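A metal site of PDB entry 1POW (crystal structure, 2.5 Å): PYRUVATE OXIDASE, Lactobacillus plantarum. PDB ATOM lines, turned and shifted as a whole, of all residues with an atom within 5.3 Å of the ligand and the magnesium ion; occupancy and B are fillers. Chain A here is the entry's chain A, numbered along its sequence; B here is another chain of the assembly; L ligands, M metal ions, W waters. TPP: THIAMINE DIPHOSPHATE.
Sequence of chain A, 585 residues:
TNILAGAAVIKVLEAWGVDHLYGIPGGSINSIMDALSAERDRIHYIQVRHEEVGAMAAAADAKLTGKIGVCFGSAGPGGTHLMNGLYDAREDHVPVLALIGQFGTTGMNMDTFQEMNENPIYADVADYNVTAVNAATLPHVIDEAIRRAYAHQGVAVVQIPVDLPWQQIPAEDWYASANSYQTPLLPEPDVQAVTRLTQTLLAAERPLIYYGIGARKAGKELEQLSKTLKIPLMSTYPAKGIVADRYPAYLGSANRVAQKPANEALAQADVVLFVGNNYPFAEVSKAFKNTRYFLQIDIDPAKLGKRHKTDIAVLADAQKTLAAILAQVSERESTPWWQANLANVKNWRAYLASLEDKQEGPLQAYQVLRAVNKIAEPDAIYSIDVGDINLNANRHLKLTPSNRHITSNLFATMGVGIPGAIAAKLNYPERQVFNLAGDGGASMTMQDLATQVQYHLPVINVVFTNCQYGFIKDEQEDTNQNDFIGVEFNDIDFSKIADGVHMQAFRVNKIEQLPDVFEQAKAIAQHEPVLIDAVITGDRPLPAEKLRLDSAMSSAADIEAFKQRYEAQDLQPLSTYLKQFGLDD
The side-chain carboxylate (OE1) of Glu 51 of chain B lies within hydrogen-bond range of a ring nitrogen (ND1) of His 81 of chain B. The backbone NH (N) of Asp 439 sits at hydrogen-bond distance from the backbone carbonyl oxygen (O) of Phe 464 (3.2 Å). ND2 of Asn 84 is in hydrogen-bond range of NE2 of His 81 of chain B (3.3 Å). The side-chain amide nitrogen (NE2) of Gln 114 of chain B lies within hydrogen-bond range of the backbone carbonyl oxygen (O) of Phe 411 (2.9 Å). The backbone NH (N) of Cys 467 lies within hydrogen-bond range of the side-chain carboxylate (OD2) of Asp 439, 2.8 Å away. OG1 of Thr 413 is in hydrogen-bond range of ND2 of Asn 84 (2.8 Å). The side-chain amide nitrogen (ND2) of Asn 84 is in hydrogen-bond range of the backbone carbonyl oxygen (O) of Pro 77 of chain B (3.1 Å).
O of Ala 412 lies within hydrogen-bond range of N4' of the ligand, at 2.8 Å. The backbone NH of Phe 471 sits at hydrogen-bond distance from an oxygen (O1B) of the ligand (2.9 Å). An oxygen (O2A) of the ligand sits at hydrogen-bond distance from the backbone NH of Gly 440, at 3.4 Å. An oxygen (O2A) of the ligand lies within hydrogen-bond range of the backbone NH (N) of Gly 441, 2.9 Å away. The backbone NH of Asp 388 lies within hydrogen-bond range of an oxygen (O1B) of the ligand, at 3.3 Å. A nitrogen (N4') of the ligand lies close to the side-chain amide nitrogen (NE2) of Gln 114 of chain B (3.4 Å). The side-chain carboxylate of Glu 51 of chain B is in hydrogen-bond range of a nitrogen (N1') of the ligand, 2.7 Å away. N of Gly 470 sits at hydrogen-bond distance from O1B of the ligand (3.1 Å).
Water W2 lies within hydrogen-bond range of O2B of the ligand (2.7 Å), N of Ile 389 (3.1 Å) and N of Asp 388 (3.2 Å). Water W1 lies within hydrogen-bond range of O of Val 386, O2A of the ligand and N of Gly 438.
The magnesium ion is bound by an oxygen (O3B) of the ligand (1.9 Å), an oxygen (O1A) of the ligand (1.9 Å), the backbone carbonyl oxygen (O) of Gln 468 (2.0 Å), the side-chain carboxylate (OD1) of Asp 439 (2.0 Å) and the side-chain amide oxygen (OD1) of Asn 466 (2.0 Å).
Val 386 touches the ligand. Gly 387 touches the ligand. OG1 of Thr 413 touches CM2 of the ligand, 3.8 Å away. Met 414 touches the ligand (CE to O2A, 3.4 Å). Gly 438 touches the ligand (C to O2A, 3.9 Å). Met 444 touches the ligand. Tyr 469 touches the ligand. Ile 472 touches the ligand. CG2 of Ile 24 of chain B touches CM4 of the ligand, at 3.8 Å. O of Pro 25 of chain B touches CM4 of the ligand, at 3.5 Å. Ser 74 of chain B touches the ligand (OG to C6', 3.4 Å). CG of Pro 77 of chain B touches N3' of the ligand, at 3.4 Å. His 81 of chain B touches the ligand (ND1 to CM2, 3.5 Å). Within 4 Å of the ligand: Val 386, Gly 387, Asp 388, Ala 412, Thr 413, Met 414, Gly 438, Asp 439, Gly 440, Gly 441, Met 444, Asn 466, Gln 468, Tyr 469, Gly 470, Phe 471, Ile 472, Ile 24 of chain B, Pro 25 of chain B, Glu 51 of chain B, Ser 74 of chain B, Pro 77 of chain B, His 81 of chain B and Gln 114 of chain B.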
ATOM      1  N   ASN A  84     -22.794   2.589 -38.443  1.00  0.00           N
ATOM      2  CA  ASN A  84     -22.632   2.860 -37.024  1.00  0.00           C
ATOM      3  C   ASN A  84     -23.839   2.478 -36.218  1.00  0.00           C
ATOM      4  O   ASN A  84     -23.689   1.980 -35.107  1.00  0.00           O
ATOM      5  CB  ASN A  84     -22.301   4.327 -36.809  1.00  0.00           C
ATOM      6  CG  ASN A  84     -20.801   4.567 -36.959  1.00  0.00           C
ATOM      7  OD1 ASN A  84     -20.185   4.311 -37.997  1.00  0.00           O
ATOM      8  ND2 ASN A  84     -20.075   5.094 -35.980  1.00  0.00           N
ATOM      9  N   VAL A 386     -21.831  10.226 -26.145  1.00  0.00           N
ATOM     10  CA  VAL A 386     -20.697   9.425 -25.673  1.00  0.00           C
ATOM     11  C   VAL A 386     -19.586  10.435 -25.474  1.00  0.00           C
ATOM     12  O   VAL A 386     -19.378  11.271 -26.360  1.00  0.00           O
ATOM     13  CB  VAL A 386     -20.289   8.365 -26.718  1.00  0.00           C
ATOM     14  CG1 VAL A 386     -18.945   7.732 -26.401  1.00  0.00           C
ATOM     15  CG2 VAL A 386     -21.292   7.235 -26.695  1.00  0.00           C
ATOM     16  N   GLY A 387     -18.906  10.355 -24.344  1.00  0.00           N
ATOM     17  CA  GLY A 387     -17.842  11.289 -24.042  1.00  0.00           C
ATOM     18  C   GLY A 387     -17.894  11.592 -22.571  1.00  0.00           C
ATOM     19  O   GLY A 387     -18.343  10.747 -21.780  1.00  0.00           O
ATOM     20  N   ASP A 388     -17.491  12.778 -22.121  1.00  0.00           N
ATOM     21  CA  ASP A 388     -17.526  13.087 -20.704  1.00  0.00           C
ATOM     22  C   ASP A 388     -18.933  13.051 -20.164  1.00  0.00           C
ATOM     23  O   ASP A 388     -19.132  12.773 -18.976  1.00  0.00           O
ATOM     24  CB  ASP A 388     -16.981  14.463 -20.406  1.00  0.00           C
ATOM     25  CG  ASP A 388     -15.475  14.587 -20.185  1.00  0.00           C
ATOM     26  OD1 ASP A 388     -14.792  13.588 -19.916  1.00  0.00           O
ATOM     27  OD2 ASP A 388     -15.002  15.721 -20.268  1.00  0.00           O
ATOM     28  N   ILE A 389     -19.944  13.297 -21.024  1.00  0.00           N
ATOM     29  CA  ILE A 389     -21.329  13.277 -20.586  1.00  0.00           C
ATOM     30  C   ILE A 389     -21.710  11.931 -20.001  1.00  0.00           C
ATOM     31  O   ILE A 389     -22.577  11.911 -19.120  1.00  0.00           O
ATOM     32  CB  ILE A 389     -22.271  13.690 -21.798  1.00  0.00           C
ATOM     33  CG1 ILE A 389     -23.697  13.795 -21.254  1.00  0.00           C
ATOM     34  CG2 ILE A 389     -22.240  12.712 -22.963  1.00  0.00           C
ATOM     35  CD1 ILE A 389     -23.944  14.807 -20.105  1.00  0.00           C
ATOM     36  N   PHE A 411     -20.096  -0.237 -28.339  1.00  0.00           N
ATOM     37  CA  PHE A 411     -19.519   0.209 -29.593  1.00  0.00           C
ATOM     38  C   PHE A 411     -19.147   1.649 -29.345  1.00  0.00           C
ATOM     39  O   PHE A 411     -18.166   2.144 -29.883  1.00  0.00           O
ATOM     40  CB  PHE A 411     -20.545   0.120 -30.709  1.00  0.00           C
ATOM     41  CG  PHE A 411     -19.973   0.295 -32.108  1.00  0.00           C
ATOM     42  CD1 PHE A 411     -18.926  -0.490 -32.524  1.00  0.00           C
ATOM     43  CD2 PHE A 411     -20.532   1.235 -32.952  1.00  0.00           C
ATOM     44  CE1 PHE A 411     -18.425  -0.338 -33.805  1.00  0.00           C
ATOM     45  CE2 PHE A 411     -20.029   1.396 -34.222  1.00  0.00           C
ATOM     46  CZ  PHE A 411     -18.980   0.601 -34.640  1.00  0.00           C
ATOM     47  N   ALA A 412     -19.963   2.332 -28.556  1.00  0.00           N
ATOM     48  CA  ALA A 412     -19.737   3.689 -28.105  1.00  0.00           C
ATOM     49  C   ALA A 412     -19.567   4.707 -29.214  1.00  0.00           C
ATOM     50  O   ALA A 412     -18.605   5.470 -29.274  1.00  0.00           O
ATOM     51  CB  ALA A 412     -18.515   3.738 -27.191  1.00  0.00           C
ATOM     52  N   THR A 413     -20.549   4.714 -30.110  1.00  0.00           N
ATOM     53  CA  THR A 413     -20.526   5.679 -31.175  1.00  0.00           C
ATOM     54  C   THR A 413     -21.113   6.979 -30.685  1.00  0.00           C
ATOM     55  O   THR A 413     -22.186   7.079 -30.073  1.00  0.00           O
ATOM     56  CB  THR A 413     -21.292   5.092 -32.385  1.00  0.00           C
ATOM     57  OG1 THR A 413     -21.017   5.994 -33.454  1.00  0.00           O
ATOM     58  CG2 THR A 413     -22.771   4.878 -32.177  1.00  0.00           C
ATOM     59  N   MET A 414     -20.364   8.042 -30.958  1.00  0.00           N
ATOM     60  CA  MET A 414     -20.855   9.384 -30.750  1.00  0.00           C
ATOM     61  C   MET A 414     -21.940   9.530 -31.800  1.00  0.00           C
ATOM     62  O   MET A 414     -21.999   8.737 -32.748  1.00  0.00           O
ATOM     63  CB  MET A 414     -19.769  10.415 -31.005  1.00  0.00           C
ATOM     64  CG  MET A 414     -18.553  10.279 -30.130  1.00  0.00           C
ATOM     65  SD  MET A 414     -17.216  11.331 -30.753  1.00  0.00           S
ATOM     66  CE  MET A 414     -17.884  12.911 -30.403  1.00  0.00           C
ATOM     67  N   GLY A 438     -22.563  16.033 -25.784  1.00  0.00           N
ATOM     68  CA  GLY A 438     -21.443  16.940 -25.846  1.00  0.00           C
ATOM     69  C   GLY A 438     -21.450  17.538 -27.239  1.00  0.00           C
ATOM     70  O   GLY A 438     -22.061  16.971 -28.169  1.00  0.00           O
ATOM     71  N   ASP A 439     -20.802  18.679 -27.419  1.00  0.00           N
ATOM     72  CA  ASP A 439     -20.632  19.331 -28.714  1.00  0.00           C
ATOM     73  C   ASP A 439     -20.062  18.474 -29.841  1.00  0.00           C
ATOM     74  O   ASP A 439     -20.589  18.576 -30.964  1.00  0.00           O
ATOM     75  CB  ASP A 439     -19.741  20.574 -28.567  1.00  0.00           C
ATOM     76  CG  ASP A 439     -18.419  20.535 -27.804  1.00  0.00           C
ATOM     77  OD1 ASP A 439     -17.907  19.490 -27.350  1.00  0.00           O
ATOM     78  OD2 ASP A 439     -17.878  21.592 -27.619  1.00  0.00           O
ATOM     79  N   GLY A 440     -19.070  17.597 -29.624  1.00  0.00           N
ATOM     80  CA  GLY A 440     -18.507  16.779 -30.690  1.00  0.00           C
ATOM     81  C   GLY A 440     -19.530  15.750 -31.144  1.00  0.00           C
ATOM     82  O   GLY A 440     -19.752  15.498 -32.323  1.00  0.00           O
ATOM     83  N   GLY A 441     -20.210  15.151 -30.170  1.00  0.00           N
ATOM     84  CA  GLY A 441     -21.258  14.181 -30.425  1.00  0.00           C
ATOM     85  C   GLY A 441     -22.461  14.812 -31.106  1.00  0.00           C
ATOM     86  O   GLY A 441     -22.999  14.236 -32.042  1.00  0.00           O
ATOM     87  N   ALA A 442     -22.899  15.984 -30.659  1.00  0.00           N
ATOM     88  CA  ALA A 442     -24.018  16.679 -31.270  1.00  0.00           C
ATOM     89  C   ALA A 442     -23.662  17.161 -32.663  1.00  0.00           C
ATOM     90  O   ALA A 442     -24.548  17.158 -33.521  1.00  0.00           O
ATOM     91  CB  ALA A 442     -24.408  17.893 -30.435  1.00  0.00           C
ATOM     92  N   MET A 444     -21.834  15.671 -35.017  1.00  0.00           N
ATOM     93  CA  MET A 444     -21.942  14.591 -35.982  1.00  0.00           C
ATOM     94  C   MET A 444     -23.365  14.273 -36.440  1.00  0.00           C
ATOM     95  O   MET A 444     -23.523  13.701 -37.518  1.00  0.00           O
ATOM     96  CB  MET A 444     -21.353  13.305 -35.431  1.00  0.00           C
ATOM     97  CG  MET A 444     -19.938  13.412 -34.943  1.00  0.00           C
ATOM     98  SD  MET A 444     -19.239  11.766 -34.660  1.00  0.00           S
ATOM     99  CE  MET A 444     -17.548  12.236 -34.507  1.00  0.00           C
ATOM    100  N   PHE A 464     -23.499  20.369 -24.379  1.00  0.00           N
ATOM    101  CA  PHE A 464     -22.443  20.741 -23.464  1.00  0.00           C
ATOM    102  C   PHE A 464     -21.259  21.234 -24.276  1.00  0.00           C
ATOM    103  O   PHE A 464     -20.432  20.415 -24.743  1.00  0.00           O
ATOM    104  CB  PHE A 464     -22.066  19.521 -22.655  1.00  0.00           C
ATOM    105  CG  PHE A 464     -23.093  19.133 -21.607  1.00  0.00           C
ATOM    106  CD1 PHE A 464     -24.268  18.509 -21.972  1.00  0.00           C
ATOM    107  CD2 PHE A 464     -22.842  19.449 -20.281  1.00  0.00           C
ATOM    108  CE1 PHE A 464     -25.200  18.193 -20.986  1.00  0.00           C
ATOM    109  CE2 PHE A 464     -23.780  19.125 -19.313  1.00  0.00           C
ATOM    110  CZ  PHE A 464     -24.951  18.500 -19.670  1.00  0.00           C
ATOM    111  N   ASN A 466     -17.843  22.657 -24.793  1.00  0.00           N
ATOM    112  CA  ASN A 466     -16.536  22.848 -24.196  1.00  0.00           C
ATOM    113  C   ASN A 466     -15.473  23.128 -25.235  1.00  0.00           C
ATOM    114  O   ASN A 466     -14.321  23.300 -24.873  1.00  0.00           O
ATOM    115  CB  ASN A 466     -16.121  21.624 -23.363  1.00  0.00           C
ATOM    116  CG  ASN A 466     -16.140  20.199 -23.909  1.00  0.00           C
ATOM    117  OD1 ASN A 466     -16.532  19.811 -25.034  1.00  0.00           O
ATOM    118  ND2 ASN A 466     -15.697  19.287 -23.057  1.00  0.00           N
ATOM    119  N   CYS A 467     -15.803  23.187 -26.537  1.00  0.00           N
ATOM    120  CA  CYS A 467     -14.870  23.431 -27.642  1.00  0.00           C
ATOM    121  C   CYS A 467     -13.695  22.462 -27.645  1.00  0.00           C
ATOM    122  O   CYS A 467     -12.558  22.688 -28.096  1.00  0.00           O
ATOM    123  CB  CYS A 467     -14.358  24.880 -27.597  1.00  0.00           C
ATOM    124  SG  CYS A 467     -15.678  26.109 -27.779  1.00  0.00           S
ATOM    125  N   GLN A 468     -14.075  21.264 -27.215  1.00  0.00           N
ATOM    126  CA  GLN A 468     -13.154  20.165 -27.047  1.00  0.00           C
ATOM    127  C   GLN A 468     -13.910  18.861 -27.168  1.00  0.00           C
ATOM    128  O   GLN A 468     -15.141  18.726 -26.935  1.00  0.00           O
ATOM    129  CB  GLN A 468     -12.531  20.113 -25.667  1.00  0.00           C
ATOM    130  CG  GLN A 468     -11.635  21.196 -25.140  1.00  0.00           C
ATOM    131  CD  GLN A 468     -11.344  21.025 -23.660  1.00  0.00           C
ATOM    132  OE1 GLN A 468     -11.160  21.998 -22.947  1.00  0.00           O
ATOM    133  NE2 GLN A 468     -11.251  19.856 -23.046  1.00  0.00           N
ATOM    134  N   TYR A 469     -13.026  17.907 -27.409  1.00  0.00           N
ATOM    135  CA  TYR A 469     -13.294  16.491 -27.313  1.00  0.00           C
ATOM    136  C   TYR A 469     -12.650  16.256 -25.940  1.00  0.00           C
ATOM    137  O   TYR A 469     -11.499  15.811 -25.841  1.00  0.00           O
ATOM    138  CB  TYR A 469     -12.538  15.716 -28.415  1.00  0.00           C
ATOM    139  CG  TYR A 469     -13.090  15.826 -29.822  1.00  0.00           C
ATOM    140  CD1 TYR A 469     -14.454  15.760 -30.073  1.00  0.00           C
ATOM    141  CD2 TYR A 469     -12.206  16.001 -30.867  1.00  0.00           C
ATOM    142  CE1 TYR A 469     -14.934  15.870 -31.370  1.00  0.00           C
ATOM    143  CE2 TYR A 469     -12.665  16.104 -32.154  1.00  0.00           C
ATOM    144  CZ  TYR A 469     -14.027  16.047 -32.394  1.00  0.00           C
ATOM    145  OH  TYR A 469     -14.486  16.195 -33.691  1.00  0.00           O
ATOM    146  N   GLY A 470     -13.376  16.554 -24.850  1.00  0.00           N
ATOM    147  CA  GLY A 470     -12.845  16.544 -23.497  1.00  0.00           C
ATOM    148  C   GLY A 470     -12.339  15.156 -23.087  1.00  0.00           C
ATOM    149  O   GLY A 470     -11.216  15.039 -22.548  1.00  0.00           O
ATOM    150  N   PHE A 471     -13.105  14.100 -23.399  1.00  0.00           N
ATOM    151  CA  PHE A 471     -12.730  12.726 -23.041  1.00  0.00           C
ATOM    152  C   PHE A 471     -11.379  12.308 -23.624  1.00  0.00           C
ATOM    153  O   PHE A 471     -10.606  11.616 -22.958  1.00  0.00           O
ATOM    154  CB  PHE A 471     -13.818  11.771 -23.536  1.00  0.00           C
ATOM    155  CG  PHE A 471     -14.047  10.550 -22.665  1.00  0.00           C
ATOM    156  CD1 PHE A 471     -14.423  10.700 -21.328  1.00  0.00           C
ATOM    157  CD2 PHE A 471     -13.900   9.286 -23.183  1.00  0.00           C
ATOM    158  CE1 PHE A 471     -14.650   9.580 -20.534  1.00  0.00           C
ATOM    159  CE2 PHE A 471     -14.117   8.178 -22.383  1.00  0.00           C
ATOM    160  CZ  PHE A 471     -14.495   8.319 -21.057  1.00  0.00           C
ATOM    161  N   ILE A 472     -11.053  12.767 -24.841  1.00  0.00           N
ATOM    162  CA  ILE A 472      -9.790  12.435 -25.499  1.00  0.00           C
ATOM    163  C   ILE A 472      -8.667  13.305 -24.957  1.00  0.00           C
ATOM    164  O   ILE A 472      -7.560  12.794 -24.699  1.00  0.00           O
ATOM    165  CB  ILE A 472      -9.900  12.627 -27.033  1.00  0.00           C
ATOM    166  CG1 ILE A 472     -11.088  11.863 -27.569  1.00  0.00           C
ATOM    167  CG2 ILE A 472      -8.649  12.114 -27.713  1.00  0.00           C
ATOM    168  CD1 ILE A 472     -11.221  10.383 -27.116  1.00  0.00           C
ATOM    169  N   PHE A 489     -11.012  22.752 -30.568  1.00  0.00           N
ATOM    170  CA  PHE A 489     -11.485  23.212 -31.856  1.00  0.00           C
ATOM    171  C   PHE A 489     -12.352  24.452 -31.796  1.00  0.00           C
ATOM    172  O   PHE A 489     -12.647  24.976 -30.720  1.00  0.00           O
ATOM    173  CB  PHE A 489     -12.249  22.072 -32.539  1.00  0.00           C
ATOM    174  CG  PHE A 489     -13.363  21.390 -31.739  1.00  0.00           C
ATOM    175  CD1 PHE A 489     -14.546  22.035 -31.458  1.00  0.00           C
ATOM    176  CD2 PHE A 489     -13.172  20.077 -31.322  1.00  0.00           C
ATOM    177  CE1 PHE A 489     -15.544  21.386 -30.755  1.00  0.00           C
ATOM    178  CE2 PHE A 489     -14.170  19.441 -30.631  1.00  0.00           C
ATOM    179  CZ  PHE A 489     -15.353  20.086 -30.349  1.00  0.00           C
ATOM    180  N   ILE B  24     -10.132  12.184 -36.697  1.00  0.00           N
ATOM    181  CA  ILE B  24     -10.603  12.606 -35.378  1.00  0.00           C
ATOM    182  C   ILE B  24      -9.804  11.745 -34.412  1.00  0.00           C
ATOM    183  O   ILE B  24      -9.745  10.536 -34.650  1.00  0.00           O
ATOM    184  CB  ILE B  24     -12.141  12.340 -35.208  1.00  0.00           C
ATOM    185  CG1 ILE B  24     -12.893  13.298 -36.105  1.00  0.00           C
ATOM    186  CG2 ILE B  24     -12.609  12.536 -33.761  1.00  0.00           C
ATOM    187  CD1 ILE B  24     -14.411  13.147 -36.056  1.00  0.00           C
ATOM    188  N   PRO B  25      -9.166  12.271 -33.350  1.00  0.00           N
ATOM    189  CA  PRO B  25      -8.425  11.480 -32.395  1.00  0.00           C
ATOM    190  C   PRO B  25      -9.328  10.529 -31.585  1.00  0.00           C
ATOM    191  O   PRO B  25     -10.553  10.615 -31.599  1.00  0.00           O
ATOM    192  CB  PRO B  25      -7.707  12.531 -31.552  1.00  0.00           C
ATOM    193  CG  PRO B  25      -8.679  13.678 -31.553  1.00  0.00           C
ATOM    194  CD  PRO B  25      -9.127  13.688 -32.998  1.00  0.00           C
ATOM    195  N   GLY B  26      -8.697   9.626 -30.871  1.00  0.00           N
ATOM    196  CA  GLY B  26      -9.364   8.683 -30.020  1.00  0.00           C
ATOM    197  C   GLY B  26      -8.266   7.954 -29.273  1.00  0.00           C
ATOM    198  O   GLY B  26      -7.119   7.907 -29.730  1.00  0.00           O
ATOM    199  N   GLU B  51     -15.953  11.548 -39.392  1.00  0.00           N
ATOM    200  CA  GLU B  51     -14.914  10.809 -40.100  1.00  0.00           C
ATOM    201  C   GLU B  51     -15.139  10.476 -41.567  1.00  0.00           C
ATOM    202  O   GLU B  51     -14.163  10.307 -42.299  1.00  0.00           O
ATOM    203  CB  GLU B  51     -14.600   9.479 -39.420  1.00  0.00           C
ATOM    204  CG  GLU B  51     -14.005   9.553 -38.020  1.00  0.00           C
ATOM    205  CD  GLU B  51     -14.952   9.624 -36.815  1.00  0.00           C
ATOM    206  OE1 GLU B  51     -16.149   9.848 -36.943  1.00  0.00           O
ATOM    207  OE2 GLU B  51     -14.477   9.465 -35.700  1.00  0.00           O
ATOM    208  N   SER B  74     -10.589   6.169 -35.352  1.00  0.00           N
ATOM    209  CA  SER B  74     -10.348   5.355 -34.177  1.00  0.00           C
ATOM    210  C   SER B  74     -11.084   4.012 -34.288  1.00  0.00           C
ATOM    211  O   SER B  74     -11.872   3.774 -35.210  1.00  0.00           O
ATOM    212  CB  SER B  74     -10.798   6.141 -32.947  1.00  0.00           C
ATOM    213  OG  SER B  74     -12.049   6.794 -33.120  1.00  0.00           O
ATOM    214  N   PRO B  77     -16.397   2.715 -34.016  1.00  0.00           N
ATOM    215  CA  PRO B  77     -17.181   3.756 -34.686  1.00  0.00           C
ATOM    216  C   PRO B  77     -16.438   4.774 -35.541  1.00  0.00           C
ATOM    217  O   PRO B  77     -16.999   5.305 -36.515  1.00  0.00           O
ATOM    218  CB  PRO B  77     -17.961   4.364 -33.531  1.00  0.00           C
ATOM    219  CG  PRO B  77     -17.090   4.177 -32.328  1.00  0.00           C
ATOM    220  CD  PRO B  77     -16.632   2.757 -32.567  1.00  0.00           C
ATOM    221  N   GLY B  78     -15.176   5.077 -35.190  1.00  0.00           N
ATOM    222  CA  GLY B  78     -14.350   5.988 -35.970  1.00  0.00           C
ATOM    223  C   GLY B  78     -14.079   5.422 -37.344  1.00  0.00           C
ATOM    224  O   GLY B  78     -14.246   6.088 -38.359  1.00  0.00           O
ATOM    225  N   HIS B  81     -17.332   4.901 -39.688  1.00  0.00           N
ATOM    226  CA  HIS B  81     -17.710   6.165 -40.289  1.00  0.00           C
ATOM    227  C   HIS B  81     -16.987   6.464 -41.607  1.00  0.00           C
ATOM    228  O   HIS B  81     -17.522   7.179 -42.461  1.00  0.00           O
ATOM    229  CB  HIS B  81     -17.433   7.305 -39.324  1.00  0.00           C
ATOM    230  CG  HIS B  81     -18.617   7.755 -38.500  1.00  0.00           C
ATOM    231  ND1 HIS B  81     -18.662   8.690 -37.569  1.00  0.00           N
ATOM    232  CD2 HIS B  81     -19.878   7.253 -38.596  1.00  0.00           C
ATOM    233  CE1 HIS B  81     -19.875   8.768 -37.098  1.00  0.00           C
ATOM    234  NE2 HIS B  81     -20.597   7.895 -37.726  1.00  0.00           N
ATOM    235  N   GLN B 114     -14.746  -1.345 -26.638  1.00  0.00           N
ATOM    236  CA  GLN B 114     -14.550  -0.893 -28.012  1.00  0.00           C
ATOM    237  C   GLN B 114     -13.501  -1.699 -28.797  1.00  0.00           C
ATOM    238  O   GLN B 114     -12.881  -1.233 -29.777  1.00  0.00           O
ATOM    239  CB  GLN B 114     -14.199   0.612 -27.956  1.00  0.00           C
ATOM    240  CG  GLN B 114     -14.424   1.417 -29.220  1.00  0.00           C
ATOM    241  CD  GLN B 114     -14.518   2.915 -28.940  1.00  0.00           C
ATOM    242  OE1 GLN B 114     -13.577   3.580 -28.488  1.00  0.00           O
ATOM    243  NE2 GLN B 114     -15.679   3.501 -29.177  1.00  0.00           N
HETATM  244  N1' TPP L   1     -15.690   8.747 -33.393  1.00  0.00           N
HETATM  245  C2' TPP L   1     -16.819   8.114 -33.121  1.00  0.00           C
HETATM  246  CM2 TPP L   1     -17.907   8.029 -34.191  1.00  0.00           C
HETATM  247  N3' TPP L   1     -17.005   7.555 -31.940  1.00  0.00           N
HETATM  248  C4' TPP L   1     -16.044   7.574 -30.996  1.00  0.00           C
HETATM  249  N4' TPP L   1     -16.201   6.779 -29.920  1.00  0.00           N
HETATM  250  C5' TPP L   1     -14.872   8.316 -31.219  1.00  0.00           C
HETATM  251  C6' TPP L   1     -14.684   8.831 -32.495  1.00  0.00           C
HETATM  252  C7' TPP L   1     -13.787   8.599 -30.140  1.00  0.00           C
HETATM  253  N3  TPP L   1     -14.229   9.493 -29.060  1.00  0.00           N
HETATM  254  C2  TPP L   1     -14.715   8.987 -27.950  1.00  0.00           C
HETATM  255  S1  TPP L   1     -15.210  10.220 -26.782  1.00  0.00           S
HETATM  256  C5  TPP L   1     -14.637  11.403 -27.960  1.00  0.00           C
HETATM  257  C4  TPP L   1     -14.192  10.827 -29.087  1.00  0.00           C
HETATM  258  CM4 TPP L   1     -13.683  11.580 -30.281  1.00  0.00           C
HETATM  259  C6  TPP L   1     -14.682  12.882 -27.673  1.00  0.00           C
HETATM  260  C7  TPP L   1     -16.061  13.283 -27.155  1.00  0.00           C
HETATM  261  O7  TPP L   1     -16.343  14.702 -27.597  1.00  0.00           O
HETATM  262  PA  TPP L   1     -17.582  15.474 -27.189  1.00  0.00           P
HETATM  263  O1A TPP L   1     -17.368  16.876 -27.507  1.00  0.00           O
HETATM  264  O2A TPP L   1     -18.741  14.820 -27.748  1.00  0.00           O
HETATM  265  O3A TPP L   1     -17.594  15.367 -25.572  1.00  0.00           O
HETATM  266  PB  TPP L   1     -16.734  15.971 -24.356  1.00  0.00           P
HETATM  267  O1B TPP L   1     -15.827  14.931 -23.926  1.00  0.00           O
HETATM  268  O2B TPP L   1     -17.733  16.304 -23.365  1.00  0.00           O
HETATM  269  O3B TPP L   1     -16.080  17.155 -24.893  1.00  0.00           O
HETATM  270 MG    MG M   1     -16.903  18.212 -26.181  1.00  0.00          MG
HETATM  271  O   HOH W   1     -20.884  13.601 -26.374  1.00  0.00           O
HETATM  272  O   HOH W   2     -19.531  14.379 -23.937  1.00  0.00           O
HETATM  273  O   HOH W   3     -18.794  17.732 -21.313  1.00  0.00           O
